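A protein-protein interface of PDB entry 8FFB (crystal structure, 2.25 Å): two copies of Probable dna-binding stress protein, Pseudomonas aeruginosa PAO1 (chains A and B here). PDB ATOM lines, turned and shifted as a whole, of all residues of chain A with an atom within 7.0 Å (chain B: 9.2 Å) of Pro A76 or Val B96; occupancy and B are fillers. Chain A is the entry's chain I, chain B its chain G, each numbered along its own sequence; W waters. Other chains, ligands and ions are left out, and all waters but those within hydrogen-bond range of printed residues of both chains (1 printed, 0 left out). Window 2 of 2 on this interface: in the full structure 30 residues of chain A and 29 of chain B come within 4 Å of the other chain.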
ATOM      1  N   ALA A  16     -28.027 -18.059  -1.986  1.00  0.00           N
ATOM      2  CA  ALA A  16     -27.531 -16.829  -2.597  1.00  0.00           C
ATOM      3  C   ALA A  16     -26.326 -17.093  -3.503  1.00  0.00           C
ATOM      4  O   ALA A  16     -26.173 -16.443  -4.544  1.00  0.00           O
ATOM      5  CB  ALA A  16     -27.182 -15.808  -1.514  1.00  0.00           C
ATOM      6  N   SER A  20     -26.389 -16.062  -7.342  1.00  0.00           N
ATOM      7  CA  SER A  20     -25.342 -15.209  -7.904  1.00  0.00           C
ATOM      8  C   SER A  20     -24.822 -15.752  -9.224  1.00  0.00           C
ATOM      9  O   SER A  20     -24.572 -14.983 -10.155  1.00  0.00           O
ATOM     10  CB  SER A  20     -24.185 -15.069  -6.936  1.00  0.00           C
ATOM     11  OG  SER A  20     -24.594 -14.347  -5.824  1.00  0.00           O
ATOM     12  N   ALA A  67     -31.718 -10.755  -8.651  1.00  0.00           N
ATOM     13  CA  ALA A  67     -30.977  -9.947  -7.689  1.00  0.00           C
ATOM     14  C   ALA A  67     -31.790  -9.716  -6.430  1.00  0.00           C
ATOM     15  O   ALA A  67     -31.261  -9.802  -5.311  1.00  0.00           O
ATOM     16  CB  ALA A  67     -30.590  -8.594  -8.294  1.00  0.00           C
ATOM     17  N   ILE A  70     -32.039 -12.598  -4.089  1.00  0.00           N
ATOM     18  CA  ILE A  70     -30.826 -12.623  -3.284  1.00  0.00           C
ATOM     19  C   ILE A  70     -30.958 -11.665  -2.113  1.00  0.00           C
ATOM     20  O   ILE A  70     -30.631 -12.003  -0.972  1.00  0.00           O
ATOM     21  CB  ILE A  70     -29.599 -12.281  -4.139  1.00  0.00           C
ATOM     22  CG1 ILE A  70     -29.390 -13.354  -5.192  1.00  0.00           C
ATOM     23  CG2 ILE A  70     -28.394 -12.134  -3.219  1.00  0.00           C
ATOM     24  CD1 ILE A  70     -28.257 -13.076  -6.125  1.00  0.00           C
ATOM     25  N   ARG A  71     -31.438 -10.449  -2.378  1.00  0.00           N
ATOM     26  CA  ARG A  71     -31.588  -9.479  -1.303  1.00  0.00           C
ATOM     27  C   ARG A  71     -32.580  -9.961  -0.255  1.00  0.00           C
ATOM     28  O   ARG A  71     -32.374  -9.758   0.942  1.00  0.00           O
ATOM     29  CB  ARG A  71     -32.022  -8.131  -1.873  1.00  0.00           C
ATOM     30  CG  ARG A  71     -31.015  -7.504  -2.830  1.00  0.00           C
ATOM     31  CD  ARG A  71     -29.699  -7.117  -2.152  1.00  0.00           C
ATOM     32  NE  ARG A  71     -29.840  -6.135  -1.076  1.00  0.00           N
ATOM     33  CZ  ARG A  71     -29.635  -6.376   0.219  1.00  0.00           C
ATOM     34  NH1 ARG A  71     -29.238  -7.560   0.658  1.00  0.00           N
ATOM     35  NH2 ARG A  71     -29.840  -5.405   1.101  1.00  0.00           N
ATOM     36  N   GLY A  74     -31.165 -12.114   2.321  1.00  0.00           N
ATOM     37  CA  GLY A  74     -30.285 -11.474   3.273  1.00  0.00           C
ATOM     38  C   GLY A  74     -28.841 -11.356   2.838  1.00  0.00           C
ATOM     39  O   GLY A  74     -27.951 -11.318   3.691  1.00  0.00           O
ATOM     40  N   PHE A  75     -28.571 -11.290   1.541  1.00  0.00           N
ATOM     41  CA  PHE A  75     -27.204 -11.151   1.061  1.00  0.00           C
ATOM     42  C   PHE A  75     -27.122 -10.116  -0.049  1.00  0.00           C
ATOM     43  O   PHE A  75     -28.108  -9.865  -0.753  1.00  0.00           O
ATOM     44  CB  PHE A  75     -26.662 -12.490   0.562  1.00  0.00           C
ATOM     45  CG  PHE A  75     -26.553 -13.517   1.647  1.00  0.00           C
ATOM     46  CD1 PHE A  75     -27.628 -14.333   1.951  1.00  0.00           C
ATOM     47  CD2 PHE A  75     -25.387 -13.652   2.380  1.00  0.00           C
ATOM     48  CE1 PHE A  75     -27.547 -15.273   2.957  1.00  0.00           C
ATOM     49  CE2 PHE A  75     -25.299 -14.589   3.394  1.00  0.00           C
ATOM     50  CZ  PHE A  75     -26.386 -15.403   3.679  1.00  0.00           C
ATOM     51  N   PRO A  76     -25.961  -9.490  -0.218  1.00  0.00           N
ATOM     52  CA  PRO A  76     -25.845  -8.462  -1.243  1.00  0.00           C
ATOM     53  C   PRO A  76     -25.800  -9.124  -2.596  1.00  0.00           C
ATOM     54  O   PRO A  76     -25.444 -10.297  -2.718  1.00  0.00           O
ATOM     55  CB  PRO A  76     -24.535  -7.746  -0.900  1.00  0.00           C
ATOM     56  CG  PRO A  76     -23.721  -8.765  -0.177  1.00  0.00           C
ATOM     57  CD  PRO A  76     -24.667  -9.789   0.421  1.00  0.00           C
ATOM     58  N   ALA A  77     -26.222  -8.354  -3.634  1.00  0.00           N
ATOM     59  CA  ALA A  77     -26.314  -8.923  -4.966  1.00  0.00           C
ATOM     60  C   ALA A  77     -25.133  -8.490  -5.797  1.00  0.00           C
ATOM     61  O   ALA A  77     -24.852  -7.291  -5.874  1.00  0.00           O
ATOM     62  CB  ALA A  77     -27.606  -8.489  -5.657  1.00  0.00           C
ATOM     63  N   PRO A  78     -24.441  -9.416  -6.448  1.00  0.00           N
ATOM     64  CA  PRO A  78     -23.282  -9.025  -7.249  1.00  0.00           C
ATOM     65  C   PRO A  78     -23.701  -8.226  -8.472  1.00  0.00           C
ATOM     66  O   PRO A  78     -24.719  -8.510  -9.107  1.00  0.00           O
ATOM     67  CB  PRO A  78     -22.661 -10.367  -7.638  1.00  0.00           C
ATOM     68  CG  PRO A  78     -23.799 -11.333  -7.611  1.00  0.00           C
ATOM     69  CD  PRO A  78     -24.727 -10.861  -6.542  1.00  0.00           C
ATOM     70  N   ASN B  35     -26.643  -1.870  -9.622  1.00  0.00           N
ATOM     71  CA  ASN B  35     -26.025  -2.438  -8.428  1.00  0.00           C
ATOM     72  C   ASN B  35     -26.548  -1.722  -7.186  1.00  0.00           C
ATOM     73  O   ASN B  35     -27.162  -2.330  -6.301  1.00  0.00           O
ATOM     74  CB  ASN B  35     -24.487  -2.333  -8.551  1.00  0.00           C
ATOM     75  CG  ASN B  35     -23.734  -3.021  -7.423  1.00  0.00           C
ATOM     76  OD1 ASN B  35     -24.114  -2.928  -6.267  1.00  0.00           O
ATOM     77  ND2 ASN B  35     -22.631  -3.707  -7.767  1.00  0.00           N
ATOM     78  N   PHE B  36     -26.343  -0.409  -7.121  1.00  0.00           N
ATOM     79  CA  PHE B  36     -26.738   0.324  -5.927  1.00  0.00           C
ATOM     80  C   PHE B  36     -28.247   0.236  -5.689  1.00  0.00           C
ATOM     81  O   PHE B  36     -28.701   0.168  -4.545  1.00  0.00           O
ATOM     82  CB  PHE B  36     -26.292   1.780  -6.044  1.00  0.00           C
ATOM     83  CG  PHE B  36     -24.786   1.978  -6.082  1.00  0.00           C
ATOM     84  CD1 PHE B  36     -23.903   0.912  -5.919  1.00  0.00           C
ATOM     85  CD2 PHE B  36     -24.259   3.253  -6.272  1.00  0.00           C
ATOM     86  CE1 PHE B  36     -22.517   1.107  -5.954  1.00  0.00           C
ATOM     87  CE2 PHE B  36     -22.873   3.465  -6.320  1.00  0.00           C
ATOM     88  CZ  PHE B  36     -22.000   2.388  -6.160  1.00  0.00           C
ATOM     89  N   HIS B  37     -29.038   0.258  -6.755  1.00  0.00           N
ATOM     90  CA  HIS B  37     -30.479   0.156  -6.599  1.00  0.00           C
ATOM     91  C   HIS B  37     -30.851  -1.071  -5.777  1.00  0.00           C
ATOM     92  O   HIS B  37     -31.703  -0.988  -4.891  1.00  0.00           O
ATOM     93  CB  HIS B  37     -31.120   0.129  -7.986  1.00  0.00           C
ATOM     94  CG  HIS B  37     -32.489  -0.484  -8.027  1.00  0.00           C
ATOM     95  ND1 HIS B  37     -33.645   0.243  -7.820  1.00  0.00           N
ATOM     96  CD2 HIS B  37     -32.885  -1.750  -8.295  1.00  0.00           C
ATOM     97  CE1 HIS B  37     -34.689  -0.552  -7.944  1.00  0.00           C
ATOM     98  NE2 HIS B  37     -34.257  -1.765  -8.228  1.00  0.00           N
ATOM     99  N   TRP B  38     -30.187  -2.207  -6.029  1.00  0.00           N
ATOM    100  CA  TRP B  38     -30.450  -3.435  -5.281  1.00  0.00           C
ATOM    101  C   TRP B  38     -29.916  -3.381  -3.851  1.00  0.00           C
ATOM    102  O   TRP B  38     -30.538  -3.930  -2.923  1.00  0.00           O
ATOM    103  CB  TRP B  38     -29.793  -4.626  -5.971  1.00  0.00           C
ATOM    104  CG  TRP B  38     -30.238  -4.940  -7.342  1.00  0.00           C
ATOM    105  CD1 TRP B  38     -31.476  -4.820  -7.842  1.00  0.00           C
ATOM    106  CD2 TRP B  38     -29.421  -5.466  -8.396  1.00  0.00           C
ATOM    107  NE1 TRP B  38     -31.500  -5.233  -9.157  1.00  0.00           N
ATOM    108  CE2 TRP B  38     -30.244  -5.636  -9.516  1.00  0.00           C
ATOM    109  CE3 TRP B  38     -28.073  -5.808  -8.494  1.00  0.00           C
ATOM    110  CZ2 TRP B  38     -29.767  -6.120 -10.725  1.00  0.00           C
ATOM    111  CZ3 TRP B  38     -27.599  -6.311  -9.692  1.00  0.00           C
ATOM    112  CH2 TRP B  38     -28.439  -6.452 -10.794  1.00  0.00           C
ATOM    113  N   ASN B  39     -28.718  -2.822  -3.665  1.00  0.00           N
ATOM    114  CA  ASN B  39     -27.929  -3.098  -2.462  1.00  0.00           C
ATOM    115  C   ASN B  39     -27.953  -1.970  -1.440  1.00  0.00           C
ATOM    116  O   ASN B  39     -27.469  -2.164  -0.323  1.00  0.00           O
ATOM    117  CB  ASN B  39     -26.477  -3.417  -2.850  1.00  0.00           C
ATOM    118  CG  ASN B  39     -26.338  -4.777  -3.478  1.00  0.00           C
ATOM    119  OD1 ASN B  39     -26.691  -5.794  -2.869  1.00  0.00           O
ATOM    120  ND2 ASN B  39     -25.843  -4.814  -4.715  1.00  0.00           N
ATOM    121  N   VAL B  40     -28.538  -0.824  -1.769  1.00  0.00           N
ATOM    122  CA  VAL B  40     -28.579   0.290  -0.834  1.00  0.00           C
ATOM    123  C   VAL B  40     -29.482  -0.044   0.340  1.00  0.00           C
ATOM    124  O   VAL B  40     -30.532  -0.675   0.175  1.00  0.00           O
ATOM    125  CB  VAL B  40     -29.078   1.557  -1.539  1.00  0.00           C
ATOM    126  CG1 VAL B  40     -30.522   1.342  -2.017  1.00  0.00           C
ATOM    127  CG2 VAL B  40     -28.970   2.748  -0.596  1.00  0.00           C
ATOM    128  N   THR B  41     -29.094   0.425   1.527  1.00  0.00           N
ATOM    129  CA  THR B  41     -29.870   0.277   2.749  1.00  0.00           C
ATOM    130  C   THR B  41     -29.819   1.587   3.520  1.00  0.00           C
ATOM    131  O   THR B  41     -29.086   2.519   3.169  1.00  0.00           O
ATOM    132  CB  THR B  41     -29.359  -0.863   3.650  1.00  0.00           C
ATOM    133  OG1 THR B  41     -27.982  -0.644   3.993  1.00  0.00           O
ATOM    134  CG2 THR B  41     -29.500  -2.199   2.958  1.00  0.00           C
ATOM    135  N   GLU B  93     -17.039  -0.386  -8.455  1.00  0.00           N
ATOM    136  CA  GLU B  93     -17.126  -0.542  -7.010  1.00  0.00           C
ATOM    137  C   GLU B  93     -17.516  -1.983  -6.713  1.00  0.00           C
ATOM    138  O   GLU B  93     -18.611  -2.422  -7.079  1.00  0.00           O
ATOM    139  CB  GLU B  93     -18.141   0.443  -6.429  1.00  0.00           C
ATOM    140  CG  GLU B  93     -18.607   0.126  -5.020  1.00  0.00           C
ATOM    141  CD  GLU B  93     -17.492   0.249  -4.016  1.00  0.00           C
ATOM    142  OE1 GLU B  93     -16.912   1.355  -3.937  1.00  0.00           O
ATOM    143  OE2 GLU B  93     -17.191  -0.751  -3.324  1.00  0.00           O
ATOM    144  N   GLU B  94     -16.623  -2.709  -6.049  1.00  0.00           N
ATOM    145  CA  GLU B  94     -16.820  -4.133  -5.822  1.00  0.00           C
ATOM    146  C   GLU B  94     -17.526  -4.437  -4.509  1.00  0.00           C
ATOM    147  O   GLU B  94     -17.966  -5.573  -4.307  1.00  0.00           O
ATOM    148  CB  GLU B  94     -15.468  -4.854  -5.863  1.00  0.00           C
ATOM    149  CG  GLU B  94     -14.694  -4.637  -7.162  1.00  0.00           C
ATOM    150  CD  GLU B  94     -15.355  -5.294  -8.366  1.00  0.00           C
ATOM    151  OE1 GLU B  94     -16.006  -6.360  -8.206  1.00  0.00           O
ATOM    152  OE2 GLU B  94     -15.226  -4.736  -9.473  1.00  0.00           O
ATOM    153  N   GLY B  95     -17.659  -3.462  -3.622  1.00  0.00           N
ATOM    154  CA  GLY B  95     -18.313  -3.712  -2.358  1.00  0.00           C
ATOM    155  C   GLY B  95     -19.693  -3.094  -2.269  1.00  0.00           C
ATOM    156  O   GLY B  95     -20.374  -2.904  -3.288  1.00  0.00           O
ATOM    157  N   VAL B  96     -20.106  -2.791  -1.040  1.00  0.00           N
ATOM    158  CA  VAL B  96     -21.404  -2.192  -0.762  1.00  0.00           C
ATOM    159  C   VAL B  96     -21.187  -0.956   0.098  1.00  0.00           C
ATOM    160  O   VAL B  96     -21.199  -1.046   1.330  1.00  0.00           O
ATOM    161  CB  VAL B  96     -22.347  -3.185  -0.065  1.00  0.00           C
ATOM    162  CG1 VAL B  96     -23.727  -2.578   0.082  1.00  0.00           C
ATOM    163  CG2 VAL B  96     -22.406  -4.478  -0.840  1.00  0.00           C
ATOM    164  N   PRO B  97     -21.005   0.214  -0.499  1.00  0.00           N
ATOM    165  CA  PRO B  97     -20.797   1.426   0.297  1.00  0.00           C
ATOM    166  C   PRO B  97     -22.055   1.849   1.037  1.00  0.00           C
ATOM    167  O   PRO B  97     -23.172   1.452   0.706  1.00  0.00           O
ATOM    168  CB  PRO B  97     -20.403   2.482  -0.745  1.00  0.00           C
ATOM    169  CG  PRO B  97     -20.078   1.732  -1.983  1.00  0.00           C
ATOM    170  CD  PRO B  97     -20.884   0.465  -1.939  1.00  0.00           C
ATOM    171  N   GLU B  98     -21.859   2.701   2.038  1.00  0.00           N
ATOM    172  CA  GLU B  98     -22.991   3.336   2.696  1.00  0.00           C
ATOM    173  C   GLU B  98     -23.743   4.208   1.683  1.00  0.00           C
ATOM    174  O   GLU B  98     -23.226   4.565   0.615  1.00  0.00           O
ATOM    175  CB  GLU B  98     -22.525   4.168   3.904  1.00  0.00           C
ATOM    176  CG  GLU B  98     -22.430   3.385   5.253  1.00  0.00           C
ATOM    177  N   ALA B  99     -24.985   4.549   2.033  1.00  0.00           N
ATOM    178  CA  ALA B  99     -25.852   5.259   1.098  1.00  0.00           C
ATOM    179  C   ALA B  99     -25.210   6.551   0.612  1.00  0.00           C
ATOM    180  O   ALA B  99     -25.262   6.861  -0.587  1.00  0.00           O
ATOM    181  CB  ALA B  99     -27.209   5.542   1.750  1.00  0.00           C
ATOM    182  N   GLU B 100     -24.604   7.321   1.524  1.00  0.00           N
ATOM    183  CA  GLU B 100     -24.069   8.627   1.152  1.00  0.00           C
ATOM    184  C   GLU B 100     -22.908   8.477   0.180  1.00  0.00           C
ATOM    185  O   GLU B 100     -22.742   9.290  -0.738  1.00  0.00           O
ATOM    186  CB  GLU B 100     -23.648   9.393   2.404  1.00  0.00           C
ATOM    187  N   GLU B 101     -22.133   7.408   0.332  1.00  0.00           N
ATOM    188  CA  GLU B 101     -21.029   7.150  -0.585  1.00  0.00           C
ATOM    189  C   GLU B 101     -21.534   6.641  -1.944  1.00  0.00           C
ATOM    190  O   GLU B 101     -20.996   7.021  -2.996  1.00  0.00           O
ATOM    191  CB  GLU B 101     -20.065   6.171   0.096  1.00  0.00           C
ATOM    192  CG  GLU B 101     -18.962   5.569  -0.781  1.00  0.00           C
ATOM    193  CD  GLU B 101     -17.930   6.570  -1.260  1.00  0.00           C
ATOM    194  OE1 GLU B 101     -17.945   7.743  -0.803  1.00  0.00           O
ATOM    195  OE2 GLU B 101     -17.111   6.170  -2.117  1.00  0.00           O
ATOM    196  N   MET B 102     -22.576   5.796  -1.953  1.00  0.00           N
ATOM    197  CA  MET B 102     -23.190   5.417  -3.224  1.00  0.00           C
ATOM    198  C   MET B 102     -23.573   6.646  -4.022  1.00  0.00           C
ATOM    199  O   MET B 102     -23.379   6.692  -5.240  1.00  0.00           O
ATOM    200  CB  MET B 102     -24.432   4.549  -2.999  1.00  0.00           C
ATOM    201  CG  MET B 102     -24.153   3.096  -2.765  1.00  0.00           C
ATOM    202  SD  MET B 102     -25.700   2.250  -2.381  1.00  0.00           S
ATOM    203  CE  MET B 102     -25.163   0.629  -1.885  1.00  0.00           C
ATOM    204  N   GLN B 105     -20.404   8.459  -5.592  1.00  0.00           N
ATOM    205  CA  GLN B 105     -19.884   7.717  -6.740  1.00  0.00           C
ATOM    206  C   GLN B 105     -20.757   7.901  -7.972  1.00  0.00           C
ATOM    207  O   GLN B 105     -20.252   7.869  -9.108  1.00  0.00           O
ATOM    208  CB  GLN B 105     -19.764   6.218  -6.428  1.00  0.00           C
ATOM    209  CG  GLN B 105     -18.679   5.830  -5.415  1.00  0.00           C
ATOM    210  CD  GLN B 105     -18.351   4.330  -5.434  1.00  0.00           C
ATOM    211  OE1 GLN B 105     -18.505   3.657  -6.449  1.00  0.00           O
ATOM    212  NE2 GLN B 105     -17.893   3.810  -4.310  1.00  0.00           N
HETATM  213  O   HOH W   1     -31.265  -3.279  -0.399  1.00  0.00           O
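Water W1 lies within hydrogen-bond range of O of Trp B38 (2.7 Å), O of Val B40 (2.8 Å) and NH2 of Arg A71 (3.0 Å).
No position is printed for both chains. Of the 9 pairs that touch across the chains among the printed residues, none has its exchanged pair printed and touching as well.
Of the 18 printed residues of chain B, 4 touch a printed residue of chain A. Printed residues of chain B that touch a printed residue of chain A: Trp B38, Asn B39, Thr B41 and Val B96. Hydrophobic or aromatic side chains of chain B within 4 Å of the printed part of chain A: Trp B38 and Val B96. Along chain B the printed residues that touch a printed residue of chain A span positions 38 to 96. Hydrophobic or aromatic side chains of chain A within 4 Å of the printed part of chain B: Ala A67, Pro A76 and Ala A77. Among the printed residues, no Asp or Glu carboxylate lies within 4 Å of a Lys or Arg side-chain nitrogen of the other chain.
Pro A76 touches two residues of chain B. Val B96 touches just one residue of chain A: Pro A76. Of chain B, only Trp B38 and Asn B39 come within 4 Å of Ala A77. Of the printed residues of chain A, Asn B39 touches Arg A71 (3.4 Å), Pro A76 (3.2 Å) and Ala A77 (2.7 Å). Of the printed residues of chain A, Thr B41 touches Arg A71. Of the printed residues of chain B, Ala A67 touches Trp B38 (3.2 Å). Gly B95 touches none of the printed residues of chain A. Glu B101 touches none of the printed residues of chain A.
Ala A67 touches Trp B38. Arg A71 touches Asn B39. NH2 of Arg A71 touches CG2 of Thr B41, at 3.7 Å. OD1 of Asn B39 touches CA of Pro A76, 3.2 Å away. Pro A76 touches Val B96. Trp B38 touches Ala A77. CZ3 of Trp B38 touches O of Pro A78 (3.7 Å).
The backbone carbonyl oxygen of Trp B38 sits at hydrogen-bond distance from the guanidinium group of Arg A71. The side-chain amide oxygen (OD1) of Asn B39 is in hydrogen-bond range of the backbone NH (N) of Ala A77 (2.7 Å).
OD1 of Asn B35 lies within hydrogen-bond range of ND2 of Asn B39 (3.0 Å). The backbone carbonyl oxygen (O) of Phe A75 lies within hydrogen-bond range of the guanidinium group (NH1) of Arg A71.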
